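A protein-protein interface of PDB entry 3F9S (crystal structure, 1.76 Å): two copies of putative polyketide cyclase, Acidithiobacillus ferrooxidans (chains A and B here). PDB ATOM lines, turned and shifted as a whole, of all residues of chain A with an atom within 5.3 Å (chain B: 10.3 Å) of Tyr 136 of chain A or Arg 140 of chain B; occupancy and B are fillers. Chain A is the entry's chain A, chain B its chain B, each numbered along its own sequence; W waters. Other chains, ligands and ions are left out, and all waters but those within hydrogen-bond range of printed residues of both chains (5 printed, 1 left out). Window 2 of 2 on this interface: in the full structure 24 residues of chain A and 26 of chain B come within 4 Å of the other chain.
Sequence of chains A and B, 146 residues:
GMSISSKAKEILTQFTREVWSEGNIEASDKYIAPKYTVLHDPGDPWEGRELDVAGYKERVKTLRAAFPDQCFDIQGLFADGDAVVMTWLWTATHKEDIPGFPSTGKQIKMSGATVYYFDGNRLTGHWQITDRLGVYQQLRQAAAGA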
ATOM      1  N   ARG A 132       7.452  32.445  36.168  1.00  0.00           N
ATOM      2  CA  ARG A 132       7.022  33.036  34.918  1.00  0.00           C
ATOM      3  C   ARG A 132       6.752  31.986  33.851  1.00  0.00           C
ATOM      4  O   ARG A 132       5.860  32.177  33.018  1.00  0.00           O
ATOM      5  CB  ARG A 132       8.045  34.001  34.381  1.00  0.00           C
ATOM      6  CG  ARG A 132       8.290  35.178  35.278  1.00  0.00           C
ATOM      7  CD  ARG A 132       9.142  36.139  34.567  1.00  0.00           C
ATOM      8  NE  ARG A 132      10.451  35.535  34.338  1.00  0.00           N
ATOM      9  CZ  ARG A 132      11.310  35.923  33.402  1.00  0.00           C
ATOM     10  NH1 ARG A 132      11.046  36.917  32.563  1.00  0.00           N
ATOM     11  NH2 ARG A 132      12.466  35.297  33.319  1.00  0.00           N
ATOM     12  N   LEU A 133       7.495  30.874  33.871  1.00  0.00           N
ATOM     13  CA  LEU A 133       7.293  29.835  32.874  1.00  0.00           C
ATOM     14  C   LEU A 133       5.891  29.221  33.025  1.00  0.00           C
ATOM     15  O   LEU A 133       5.219  28.980  32.018  1.00  0.00           O
ATOM     16  CB  LEU A 133       8.369  28.749  32.929  1.00  0.00           C
ATOM     17  CG  LEU A 133       8.240  27.678  31.844  1.00  0.00           C
ATOM     18  CD1 LEU A 133       8.275  28.316  30.427  1.00  0.00           C
ATOM     19  CD2 LEU A 133       9.313  26.637  31.999  1.00  0.00           C
ATOM     20  N   GLY A 134       5.476  28.994  34.268  1.00  0.00           N
ATOM     21  CA  GLY A 134       4.138  28.516  34.605  1.00  0.00           C
ATOM     22  C   GLY A 134       3.074  29.413  34.009  1.00  0.00           C
ATOM     23  O   GLY A 134       2.189  28.936  33.314  1.00  0.00           O
ATOM     24  N   VAL A 135       3.193  30.720  34.221  1.00  0.00           N
ATOM     25  CA  VAL A 135       2.241  31.680  33.627  1.00  0.00           C
ATOM     26  C   VAL A 135       2.262  31.589  32.096  1.00  0.00           C
ATOM     27  O   VAL A 135       1.211  31.474  31.469  1.00  0.00           O
ATOM     28  CB  VAL A 135       2.525  33.137  34.099  1.00  0.00           C
ATOM     29  CG1 VAL A 135       1.585  34.148  33.442  1.00  0.00           C
ATOM     30  CG2 VAL A 135       2.372  33.223  35.581  1.00  0.00           C
ATOM     31  N   TYR A 136       3.464  31.624  31.522  1.00  0.00           N
ATOM     32  CA  TYR A 136       3.709  31.520  30.072  1.00  0.00           C
ATOM     33  C   TYR A 136       2.994  30.289  29.515  1.00  0.00           C
ATOM     34  O   TYR A 136       2.242  30.398  28.545  1.00  0.00           O
ATOM     35  CB  TYR A 136       5.234  31.486  29.851  1.00  0.00           C
ATOM     36  CG  TYR A 136       5.748  31.326  28.443  1.00  0.00           C
ATOM     37  CD1 TYR A 136       5.814  30.064  27.846  1.00  0.00           C
ATOM     38  CD2 TYR A 136       6.274  32.419  27.746  1.00  0.00           C
ATOM     39  CE1 TYR A 136       6.325  29.902  26.561  1.00  0.00           C
ATOM     40  CE2 TYR A 136       6.795  32.265  26.463  1.00  0.00           C
ATOM     41  CZ  TYR A 136       6.825  31.002  25.884  1.00  0.00           C
ATOM     42  OH  TYR A 136       7.314  30.870  24.605  1.00  0.00           O
ATOM     43  N   GLN A 137       3.183  29.147  30.172  1.00  0.00           N
ATOM     44  CA  GLN A 137       2.521  27.885  29.816  1.00  0.00           C
ATOM     45  C   GLN A 137       0.992  27.935  29.915  1.00  0.00           C
ATOM     46  O   GLN A 137       0.291  27.435  29.026  1.00  0.00           O
ATOM     47  CB  GLN A 137       3.025  26.749  30.710  1.00  0.00           C
ATOM     48  CG  GLN A 137       4.448  26.310  30.396  1.00  0.00           C
ATOM     49  CD  GLN A 137       4.990  25.324  31.415  1.00  0.00           C
ATOM     50  OE1 GLN A 137       4.426  25.151  32.492  1.00  0.00           O
ATOM     51  NE2 GLN A 137       6.100  24.679  31.079  1.00  0.00           N
ATOM     52  N   GLN A 138       0.490  28.507  31.007  1.00  0.00           N
ATOM     53  CA  GLN A 138      -0.955  28.664  31.224  1.00  0.00           C
ATOM     54  C   GLN A 138      -1.606  29.563  30.173  1.00  0.00           C
ATOM     55  O   GLN A 138      -2.725  29.279  29.731  1.00  0.00           O
ATOM     56  CB  GLN A 138      -1.250  29.234  32.604  1.00  0.00           C
ATOM     57  CG  GLN A 138      -0.934  28.309  33.759  1.00  0.00           C
ATOM     58  CD  GLN A 138      -0.950  29.085  35.053  1.00  0.00           C
ATOM     59  OE1 GLN A 138      -1.946  29.732  35.374  1.00  0.00           O
ATOM     60  NE2 GLN A 138       0.147  29.047  35.794  1.00  0.00           N
ATOM     61  N   LEU A 139      -0.919  30.639  29.796  1.00  0.00           N
ATOM     62  CA  LEU A 139      -1.382  31.526  28.721  1.00  0.00           C
ATOM     63  C   LEU A 139      -1.426  30.790  27.384  1.00  0.00           C
ATOM     64  O   LEU A 139      -2.313  31.075  26.576  1.00  0.00           O
ATOM     65  CB  LEU A 139      -0.502  32.774  28.604  1.00  0.00           C
ATOM     66  CG  LEU A 139      -0.558  33.771  29.760  1.00  0.00           C
ATOM     67  CD1 LEU A 139       0.573  34.769  29.627  1.00  0.00           C
ATOM     68  CD2 LEU A 139      -1.906  34.478  29.838  1.00  0.00           C
ATOM     69  N   ARG A 140      -0.489  29.858  27.164  1.00  0.00           N
ATOM     70  CA  ARG A 140      -0.481  29.005  25.967  1.00  0.00           C
ATOM     71  C   ARG A 140      -1.720  28.126  25.939  1.00  0.00           C
ATOM     72  O   ARG A 140      -2.372  28.046  24.892  1.00  0.00           O
ATOM     73  CB  ARG A 140       0.778  28.110  25.822  1.00  0.00           C
ATOM     74  CG  ARG A 140       2.174  28.787  25.679  1.00  0.00           C
ATOM     75  CD  ARG A 140       2.058  29.984  24.791  1.00  0.00           C
ATOM     76  NE  ARG A 140       3.254  30.583  24.192  1.00  0.00           N
ATOM     77  CZ  ARG A 140       3.912  31.676  24.601  1.00  0.00           C
ATOM     78  NH1 ARG A 140       3.612  32.324  25.734  1.00  0.00           N
ATOM     79  NH2 ARG A 140       4.936  32.113  23.862  1.00  0.00           N
ATOM     80  N   PHE B  67      22.443  19.126  32.977  1.00  0.00           N
ATOM     81  CA  PHE B  67      23.548  20.076  33.140  1.00  0.00           C
ATOM     82  C   PHE B  67      24.517  19.545  34.176  1.00  0.00           C
ATOM     83  O   PHE B  67      24.555  20.048  35.303  1.00  0.00           O
ATOM     84  CB  PHE B  67      23.019  21.452  33.527  1.00  0.00           C
ATOM     85  CG  PHE B  67      22.209  22.101  32.444  1.00  0.00           C
ATOM     86  CD1 PHE B  67      22.835  22.799  31.412  1.00  0.00           C
ATOM     87  CD2 PHE B  67      20.819  22.007  32.439  1.00  0.00           C
ATOM     88  CE1 PHE B  67      22.076  23.399  30.404  1.00  0.00           C
ATOM     89  CE2 PHE B  67      20.058  22.612  31.442  1.00  0.00           C
ATOM     90  CZ  PHE B  67      20.677  23.285  30.412  1.00  0.00           C
ATOM     91  N   HIS B  94      25.816  24.234  28.450  1.00  0.00           N
ATOM     92  CA  HIS B  94      24.912  23.440  27.661  1.00  0.00           C
ATOM     93  C   HIS B  94      25.762  22.514  26.789  1.00  0.00           C
ATOM     94  O   HIS B  94      25.864  22.673  25.593  1.00  0.00           O
ATOM     95  CB  HIS B  94      23.966  24.345  26.896  1.00  0.00           C
ATOM     96  CG  HIS B  94      22.890  23.612  26.168  1.00  0.00           C
ATOM     97  ND1 HIS B  94      22.158  24.196  25.163  1.00  0.00           N
ATOM     98  CD2 HIS B  94      22.445  22.337  26.273  1.00  0.00           C
ATOM     99  CE1 HIS B  94      21.286  23.318  24.695  1.00  0.00           C
ATOM    100  NE2 HIS B  94      21.462  22.174  25.328  1.00  0.00           N
ATOM    101  N   ILE B  98      19.655  18.278  25.623  1.00  0.00           N
ATOM    102  CA  ILE B  98      18.524  18.246  26.537  1.00  0.00           C
ATOM    103  C   ILE B  98      17.253  18.249  25.683  1.00  0.00           C
ATOM    104  O   ILE B  98      17.328  18.603  24.508  1.00  0.00           O
ATOM    105  CB  ILE B  98      18.621  19.359  27.592  1.00  0.00           C
ATOM    106  CG1 ILE B  98      18.434  20.746  26.979  1.00  0.00           C
ATOM    107  CG2 ILE B  98      19.965  19.265  28.315  1.00  0.00           C
ATOM    108  CD1 ILE B  98      18.482  21.821  28.023  1.00  0.00           C
ATOM    109  N   PRO B  99      16.097  17.850  26.255  1.00  0.00           N
ATOM    110  CA  PRO B  99      14.911  17.730  25.406  1.00  0.00           C
ATOM    111  C   PRO B  99      14.604  19.038  24.670  1.00  0.00           C
ATOM    112  O   PRO B  99      14.564  20.093  25.292  1.00  0.00           O
ATOM    113  CB  PRO B  99      13.801  17.328  26.386  1.00  0.00           C
ATOM    114  CG  PRO B  99      14.507  16.778  27.576  1.00  0.00           C
ATOM    115  CD  PRO B  99      15.794  17.524  27.660  1.00  0.00           C
ATOM    116  N   GLY B 100      14.505  18.945  23.355  1.00  0.00           N
ATOM    117  CA  GLY B 100      14.255  20.090  22.485  1.00  0.00           C
ATOM    118  C   GLY B 100      15.464  20.937  22.155  1.00  0.00           C
ATOM    119  O   GLY B 100      15.395  21.725  21.229  1.00  0.00           O
ATOM    120  N   PHE B 101      16.579  20.752  22.857  1.00  0.00           N
ATOM    121  CA  PHE B 101      17.734  21.616  22.718  1.00  0.00           C
ATOM    122  C   PHE B 101      19.058  20.852  22.698  1.00  0.00           C
ATOM    123  O   PHE B 101      19.661  20.632  23.752  1.00  0.00           O
ATOM    124  CB  PHE B 101      17.718  22.639  23.848  1.00  0.00           C
ATOM    125  CG  PHE B 101      16.526  23.525  23.830  1.00  0.00           C
ATOM    126  CD1 PHE B 101      16.433  24.528  22.875  1.00  0.00           C
ATOM    127  CD2 PHE B 101      15.475  23.352  24.744  1.00  0.00           C
ATOM    128  CE1 PHE B 101      15.334  25.374  22.840  1.00  0.00           C
ATOM    129  CE2 PHE B 101      14.374  24.191  24.712  1.00  0.00           C
ATOM    130  CZ  PHE B 101      14.302  25.205  23.751  1.00  0.00           C
ATOM    131  N   PRO B 102      19.533  20.485  21.497  1.00  0.00           N
ATOM    132  CA  PRO B 102      20.862  19.870  21.376  1.00  0.00           C
ATOM    133  C   PRO B 102      21.940  20.808  21.939  1.00  0.00           C
ATOM    134  O   PRO B 102      21.761  22.035  21.913  1.00  0.00           O
ATOM    135  CB  PRO B 102      21.026  19.664  19.867  1.00  0.00           C
ATOM    136  CG  PRO B 102      19.642  19.648  19.340  1.00  0.00           C
ATOM    137  CD  PRO B 102      18.886  20.616  20.178  1.00  0.00           C
ATOM    138  N   THR B 104      24.918  23.235  22.773  1.00  0.00           N
ATOM    139  CA  THR B 104      25.502  24.385  22.093  1.00  0.00           C
ATOM    140  C   THR B 104      26.857  24.797  22.653  1.00  0.00           C
ATOM    141  O   THR B 104      27.537  25.594  22.017  1.00  0.00           O
ATOM    142  CB  THR B 104      24.582  25.599  22.217  1.00  0.00           C
ATOM    143  OG1 THR B 104      24.514  26.013  23.590  1.00  0.00           O
ATOM    144  CG2 THR B 104      23.191  25.258  21.689  1.00  0.00           C
ATOM    145  N   LYS B 106      27.067  26.689  25.132  1.00  0.00           N
ATOM    146  CA  LYS B 106      26.859  27.995  25.712  1.00  0.00           C
ATOM    147  C   LYS B 106      26.599  27.864  27.189  1.00  0.00           C
ATOM    148  O   LYS B 106      26.175  26.798  27.650  1.00  0.00           O
ATOM    149  CB  LYS B 106      25.729  28.736  25.017  1.00  0.00           C
ATOM    150  CG  LYS B 106      26.075  28.997  23.580  1.00  0.00           C
ATOM    151  CD  LYS B 106      25.092  29.900  22.901  1.00  0.00           C
ATOM    152  CE  LYS B 106      25.600  30.289  21.519  1.00  0.00           C
ATOM    153  NZ  LYS B 106      26.813  31.166  21.534  1.00  0.00           N
ATOM    154  N   GLN B 107      26.889  28.939  27.921  1.00  0.00           N
ATOM    155  CA  GLN B 107      26.638  28.990  29.335  1.00  0.00           C
ATOM    156  C   GLN B 107      25.185  29.324  29.508  1.00  0.00           C
ATOM    157  O   GLN B 107      24.681  30.231  28.839  1.00  0.00           O
ATOM    158  CB  GLN B 107      27.446  30.074  30.061  1.00  0.00           C
ATOM    159  CG  GLN B 107      28.858  29.711  30.406  1.00  0.00           C
ATOM    160  CD  GLN B 107      28.944  28.426  31.194  1.00  0.00           C
ATOM    161  OE1 GLN B 107      28.325  28.302  32.252  1.00  0.00           O
ATOM    162  NE2 GLN B 107      29.678  27.445  30.671  1.00  0.00           N
ATOM    163  N   ILE B 108      24.518  28.556  30.353  1.00  0.00           N
ATOM    164  CA  ILE B 108      23.126  28.786  30.693  1.00  0.00           C
ATOM    165  C   ILE B 108      23.177  29.328  32.109  1.00  0.00           C
ATOM    166  O   ILE B 108      23.858  28.765  32.969  1.00  0.00           O
ATOM    167  CB  ILE B 108      22.277  27.525  30.632  1.00  0.00           C
ATOM    168  CG1 ILE B 108      22.289  26.931  29.225  1.00  0.00           C
ATOM    169  CG2 ILE B 108      20.841  27.800  31.083  1.00  0.00           C
ATOM    170  CD1 ILE B 108      21.824  27.859  28.148  1.00  0.00           C
ATOM    171  N   ASP B 131      14.212  30.306  37.881  1.00  0.00           N
ATOM    172  CA  ASP B 131      13.984  31.078  36.680  1.00  0.00           C
ATOM    173  C   ASP B 131      13.996  30.157  35.466  1.00  0.00           C
ATOM    174  O   ASP B 131      14.900  30.223  34.633  1.00  0.00           O
ATOM    175  CB  ASP B 131      15.012  32.177  36.533  1.00  0.00           C
ATOM    176  CG  ASP B 131      14.731  33.098  35.387  1.00  0.00           C
ATOM    177  OD1 ASP B 131      13.569  33.141  34.940  1.00  0.00           O
ATOM    178  OD2 ASP B 131      15.679  33.774  34.923  1.00  0.00           O
ATOM    179  N   ARG B 132      12.969  29.319  35.365  1.00  0.00           N
ATOM    180  CA  ARG B 132      12.849  28.398  34.241  1.00  0.00           C
ATOM    181  C   ARG B 132      12.603  29.116  32.948  1.00  0.00           C
ATOM    182  O   ARG B 132      13.094  28.672  31.911  1.00  0.00           O
ATOM    183  CB  ARG B 132      11.732  27.392  34.446  1.00  0.00           C
ATOM    184  CG  ARG B 132      11.979  26.455  35.612  1.00  0.00           C
ATOM    185  CD  ARG B 132      10.931  25.399  35.644  1.00  0.00           C
ATOM    186  NE  ARG B 132       9.612  25.984  35.834  1.00  0.00           N
ATOM    187  CZ  ARG B 132       8.461  25.418  35.462  1.00  0.00           C
ATOM    188  NH1 ARG B 132       8.390  24.204  34.921  1.00  0.00           N
ATOM    189  NH2 ARG B 132       7.337  26.075  35.669  1.00  0.00           N
ATOM    190  N   LEU B 133      11.815  30.191  32.977  1.00  0.00           N
ATOM    191  CA  LEU B 133      11.573  30.949  31.771  1.00  0.00           C
ATOM    192  C   LEU B 133      12.874  31.533  31.240  1.00  0.00           C
ATOM    193  O   LEU B 133      13.094  31.512  30.055  1.00  0.00           O
ATOM    194  CB  LEU B 133      10.544  32.055  31.991  1.00  0.00           C
ATOM    195  CG  LEU B 133      10.175  32.804  30.706  1.00  0.00           C
ATOM    196  CD1 LEU B 133       9.605  31.881  29.628  1.00  0.00           C
ATOM    197  CD2 LEU B 133       9.169  33.875  31.039  1.00  0.00           C
ATOM    198  N   GLY B 134      13.702  32.092  32.108  1.00  0.00           N
ATOM    199  CA  GLY B 134      15.001  32.627  31.699  1.00  0.00           C
ATOM    200  C   GLY B 134      15.833  31.585  30.977  1.00  0.00           C
ATOM    201  O   GLY B 134      16.414  31.862  29.947  1.00  0.00           O
ATOM    202  N   VAL B 135      15.875  30.371  31.512  1.00  0.00           N
ATOM    203  CA  VAL B 135      16.613  29.268  30.891  1.00  0.00           C
ATOM    204  C   VAL B 135      16.012  28.909  29.551  1.00  0.00           C
ATOM    205  O   VAL B 135      16.715  28.760  28.567  1.00  0.00           O
ATOM    206  CB  VAL B 135      16.656  28.035  31.836  1.00  0.00           C
ATOM    207  CG1 VAL B 135      17.181  26.767  31.122  1.00  0.00           C
ATOM    208  CG2 VAL B 135      17.506  28.380  33.049  1.00  0.00           C
ATOM    209  N   TYR B 136      14.697  28.808  29.523  1.00  0.00           N
ATOM    210  CA  TYR B 136      13.977  28.500  28.296  1.00  0.00           C
ATOM    211  C   TYR B 136      14.288  29.526  27.219  1.00  0.00           C
ATOM    212  O   TYR B 136      14.547  29.183  26.066  1.00  0.00           O
ATOM    213  CB  TYR B 136      12.484  28.463  28.569  1.00  0.00           C
ATOM    214  CG  TYR B 136      11.729  28.103  27.323  1.00  0.00           C
ATOM    215  CD1 TYR B 136      11.875  26.834  26.754  1.00  0.00           C
ATOM    216  CD2 TYR B 136      10.908  29.032  26.691  1.00  0.00           C
ATOM    217  CE1 TYR B 136      11.189  26.481  25.599  1.00  0.00           C
ATOM    218  CE2 TYR B 136      10.206  28.689  25.552  1.00  0.00           C
ATOM    219  CZ  TYR B 136      10.364  27.422  25.003  1.00  0.00           C
ATOM    220  OH  TYR B 136       9.679  27.109  23.866  1.00  0.00           O
ATOM    221  N   GLN B 137      14.281  30.789  27.625  1.00  0.00           N
ATOM    222  CA  GLN B 137      14.637  31.879  26.726  1.00  0.00           C
ATOM    223  C   GLN B 137      16.047  31.747  26.175  1.00  0.00           C
ATOM    224  O   GLN B 137      16.259  31.838  24.964  1.00  0.00           O
ATOM    225  CB  GLN B 137      14.491  33.208  27.441  1.00  0.00           C
ATOM    226  CG  GLN B 137      13.054  33.596  27.672  1.00  0.00           C
ATOM    227  CD  GLN B 137      12.931  34.861  28.502  1.00  0.00           C
ATOM    228  OE1 GLN B 137      13.873  35.274  29.195  1.00  0.00           O
ATOM    229  NE2 GLN B 137      11.753  35.482  28.439  1.00  0.00           N
ATOM    230  N   GLN B 138      16.996  31.490  27.062  1.00  0.00           N
ATOM    231  CA  GLN B 138      18.399  31.315  26.668  1.00  0.00           C
ATOM    232  C   GLN B 138      18.535  30.155  25.689  1.00  0.00           C
ATOM    233  O   GLN B 138      19.196  30.274  24.667  1.00  0.00           O
ATOM    234  CB  GLN B 138      19.253  31.045  27.888  1.00  0.00           C
ATOM    235  CG  GLN B 138      19.380  32.249  28.769  1.00  0.00           C
ATOM    236  CD  GLN B 138      19.983  31.878  30.067  1.00  0.00           C
ATOM    237  OE1 GLN B 138      21.142  31.489  30.112  1.00  0.00           O
ATOM    238  NE2 GLN B 138      19.226  32.016  31.138  1.00  0.00           N
ATOM    239  N   LEU B 139      17.866  29.050  25.994  1.00  0.00           N
ATOM    240  CA  LEU B 139      17.900  27.869  25.123  1.00  0.00           C
ATOM    241  C   LEU B 139      17.328  28.160  23.748  1.00  0.00           C
ATOM    242  O   LEU B 139      17.909  27.769  22.731  1.00  0.00           O
ATOM    243  CB  LEU B 139      17.144  26.708  25.766  1.00  0.00           C
ATOM    244  CG  LEU B 139      17.837  26.142  27.012  1.00  0.00           C
ATOM    245  CD1 LEU B 139      16.891  25.194  27.723  1.00  0.00           C
ATOM    246  CD2 LEU B 139      19.152  25.447  26.648  1.00  0.00           C
ATOM    247  N   ARG B 140      16.174  28.818  23.740  1.00  0.00           N
ATOM    248  CA  ARG B 140      15.521  29.249  22.499  1.00  0.00           C
ATOM    249  C   ARG B 140      16.379  30.220  21.697  1.00  0.00           C
ATOM    250  O   ARG B 140      16.473  30.098  20.481  1.00  0.00           O
ATOM    251  CB  ARG B 140      14.178  29.902  22.807  1.00  0.00           C
ATOM    252  CG  ARG B 140      13.105  28.911  23.181  1.00  0.00           C
ATOM    253  CD  ARG B 140      12.532  28.217  21.956  1.00  0.00           C
ATOM    254  NE  ARG B 140      11.969  29.198  21.023  1.00  0.00           N
ATOM    255  CZ  ARG B 140      10.754  29.756  21.076  1.00  0.00           C
ATOM    256  NH1 ARG B 140       9.874  29.446  22.021  1.00  0.00           N
ATOM    257  NH2 ARG B 140      10.417  30.653  20.152  1.00  0.00           N
ATOM    258  N   GLN B 141      16.989  31.186  22.372  1.00  0.00           N
ATOM    259  CA  GLN B 141      17.858  32.169  21.705  1.00  0.00           C
ATOM    260  C   GLN B 141      19.057  31.496  21.025  1.00  0.00           C
ATOM    261  O   GLN B 141      19.434  31.885  19.925  1.00  0.00           O
ATOM    262  CB  GLN B 141      18.330  33.252  22.688  1.00  0.00           C
ATOM    263  N   ALA B 142      19.620  30.480  21.683  1.00  0.00           N
ATOM    264  CA  ALA B 142      20.754  29.701  21.191  1.00  0.00           C
ATOM    265  C   ALA B 142      20.406  28.602  20.177  1.00  0.00           C
ATOM    266  O   ALA B 142      21.294  28.154  19.454  1.00  0.00           O
ATOM    267  CB  ALA B 142      21.491  29.066  22.368  1.00  0.00           C
ATOM    268  N   ALA B 143      19.141  28.191  20.104  1.00  0.00           N
ATOM    269  CA  ALA B 143      18.718  27.091  19.235  1.00  0.00           C
ATOM    270  C   ALA B 143      18.734  27.448  17.747  1.00  0.00           C
ATOM    271  O   ALA B 143      18.718  28.624  17.376  1.00  0.00           O
ATOM    272  CB  ALA B 143      17.348  26.600  19.651  1.00  0.00           C
HETATM  273  O   HOH W   1      14.237  36.678  31.422  1.00  0.00           O
HETATM  274  O   HOH W   2      11.763  38.142  29.961  1.00  0.00           O
HETATM  275  O   HOH W   3       7.252  28.239  23.848  1.00  0.00           O
HETATM  276  O   HOH W   4       5.050  24.341  34.954  1.00  0.00           O
HETATM  277  O   HOH W   5      11.195  33.273  36.016  1.00  0.00           O
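OD1 of Asp 131 of chain B lies within salt-bridge range of NH2 of Arg 132 of chain A.
Among the printed residues, pairs that only touch across the chains: Arg 132 of chain A with Leu 133 of chain B, Arg 132 of chain A with Gly 134 of chain B, Leu 133 of chain A with Arg 132 of chain B, Leu 133 of chain A with Leu 133 of chain B, Gly 134 of chain A with Arg 132 of chain B, Tyr 136 of chain A with Leu 133 of chain B, Tyr 136 of chain A with Tyr 136 of chain B and Tyr 136 of chain A with Arg 140 of chain B.
Of the 9 printed residues of chain A, 4 touch a printed residue of chain B. Of the 24 printed residues of chain B, 6 touch a printed residue of chain A. Printed residues of chain B that touch a printed residue of chain A: Asp 131, Arg 132, Leu 133, Gly 134, Tyr 136 and Arg 140. Along chain B the printed residues that touch a printed residue of chain A span positions 131 to 140. Among the printed residues, 9 pairs touch across the chains. Among the printed residues, Asp or Glu carboxylates within 4 Å of a Lys or Arg side-chain nitrogen of the other chain: Arg 132 of chain A with Asp 131 of chain B.
Water W5 bridges OD1 of Asp 131 of chain B (2.6 Å) and NE of Arg 132 of chain A (2.9 Å). Water W1 bridges the side-chain amide oxygen of Gln 137 of chain B (2.7 Å) and the guanidinium group of Arg 132 of chain A (2.9 Å). Water W4 lies within hydrogen-bond range of OE1 of Gln 137 of chain A (2.7 Å) and NH2 of Arg 132 of chain B (3.0 Å). Water W3 lies within hydrogen-bond range of the side-chain hydroxyl (OH) of Tyr 136 of chain B (2.7 Å), the side-chain hydroxyl (OH) of Tyr 136 of chain A (2.7 Å) and the guanidinium group (NH1) of Arg 140 of chain B (3.4 Å). Water W2 bridges NH1 of Arg 132 of chain A (3.0 Å) and NE2 of Gln 137 of chain B (3.1 Å).
O of Gly 134 of chain A lies within hydrogen-bond range of NE2 of Gln 138 of chain A (3.2 Å). The guanidinium group (NH2) of Arg 140 of chain A lies within hydrogen-bond range of the side-chain hydroxyl (OH) of Tyr 136 of chain A (2.8 Å). OD1 of Asp 131 of chain B sits at hydrogen-bond distance from N of Gly 134 of chain B (3.0 Å). The side-chain amide nitrogen (NE2) of Gln 138 of chain B is in hydrogen-bond range of the backbone carbonyl oxygen (O) of Gly 134 of chain B, 3.1 Å away. The guanidinium group (NH1) of Arg 140 of chain B lies within hydrogen-bond range of the side-chain hydroxyl (OH) of Tyr 136 of chain B.
Printed residues of chain B within 4 Å of Gly 134 of chain A: Arg 132. No residue of chain B comes within 4 Å of Val 135 of chain A. Tyr 136 of chain A touches three residues of chain B. No residue of chain B comes within 4 Å of Leu 139 of chain A. Arg 140 of chain A touches none of the printed residues of chain B. Gln 107 of chain B touches none of the printed residues of chain A. Of the printed residues of chain A, Asp 131 of chain B touches Arg 132 (2.9 Å). Printed residues of chain A within 4 Å of Arg 132 of chain B: Leu 133 and Gly 134. Arg 140 of chain B touches just one residue of chain A: Tyr 136. The nearest residue of chain B that does not touch Tyr 136 of chain A is Gln 137 of chain B (6.2 Å). The nearest printed residue of chain A that does not touch Arg 140 of chain B is Arg 140 of chain A (5.9 Å). The nearest printed residue of chain A that does not touch Arg 132 of chain B is Gln 137 of chain A (4.4 Å).
Arg 132 of chain A touches Leu 133 of chain B, and with the chains exchanged Leu 133 of chain A touches Arg 132 of chain B. Arg 132 of chain A touches Gly 134 of chain B, and with the chains exchanged Gly 134 of chain A touches Arg 132 of chain B. Tyr 136 of chain A touches Leu 133 of chain B, but with the chains exchanged Leu 133 of chain A does not touch Tyr 136 of chain B (4.6 Å). Tyr 136 of chain A touches Arg 140 of chain B, but with the chains exchanged Arg 140 of chain A does not touch Tyr 136 of chain B (6.5 Å). 9 positions are printed for both chains.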
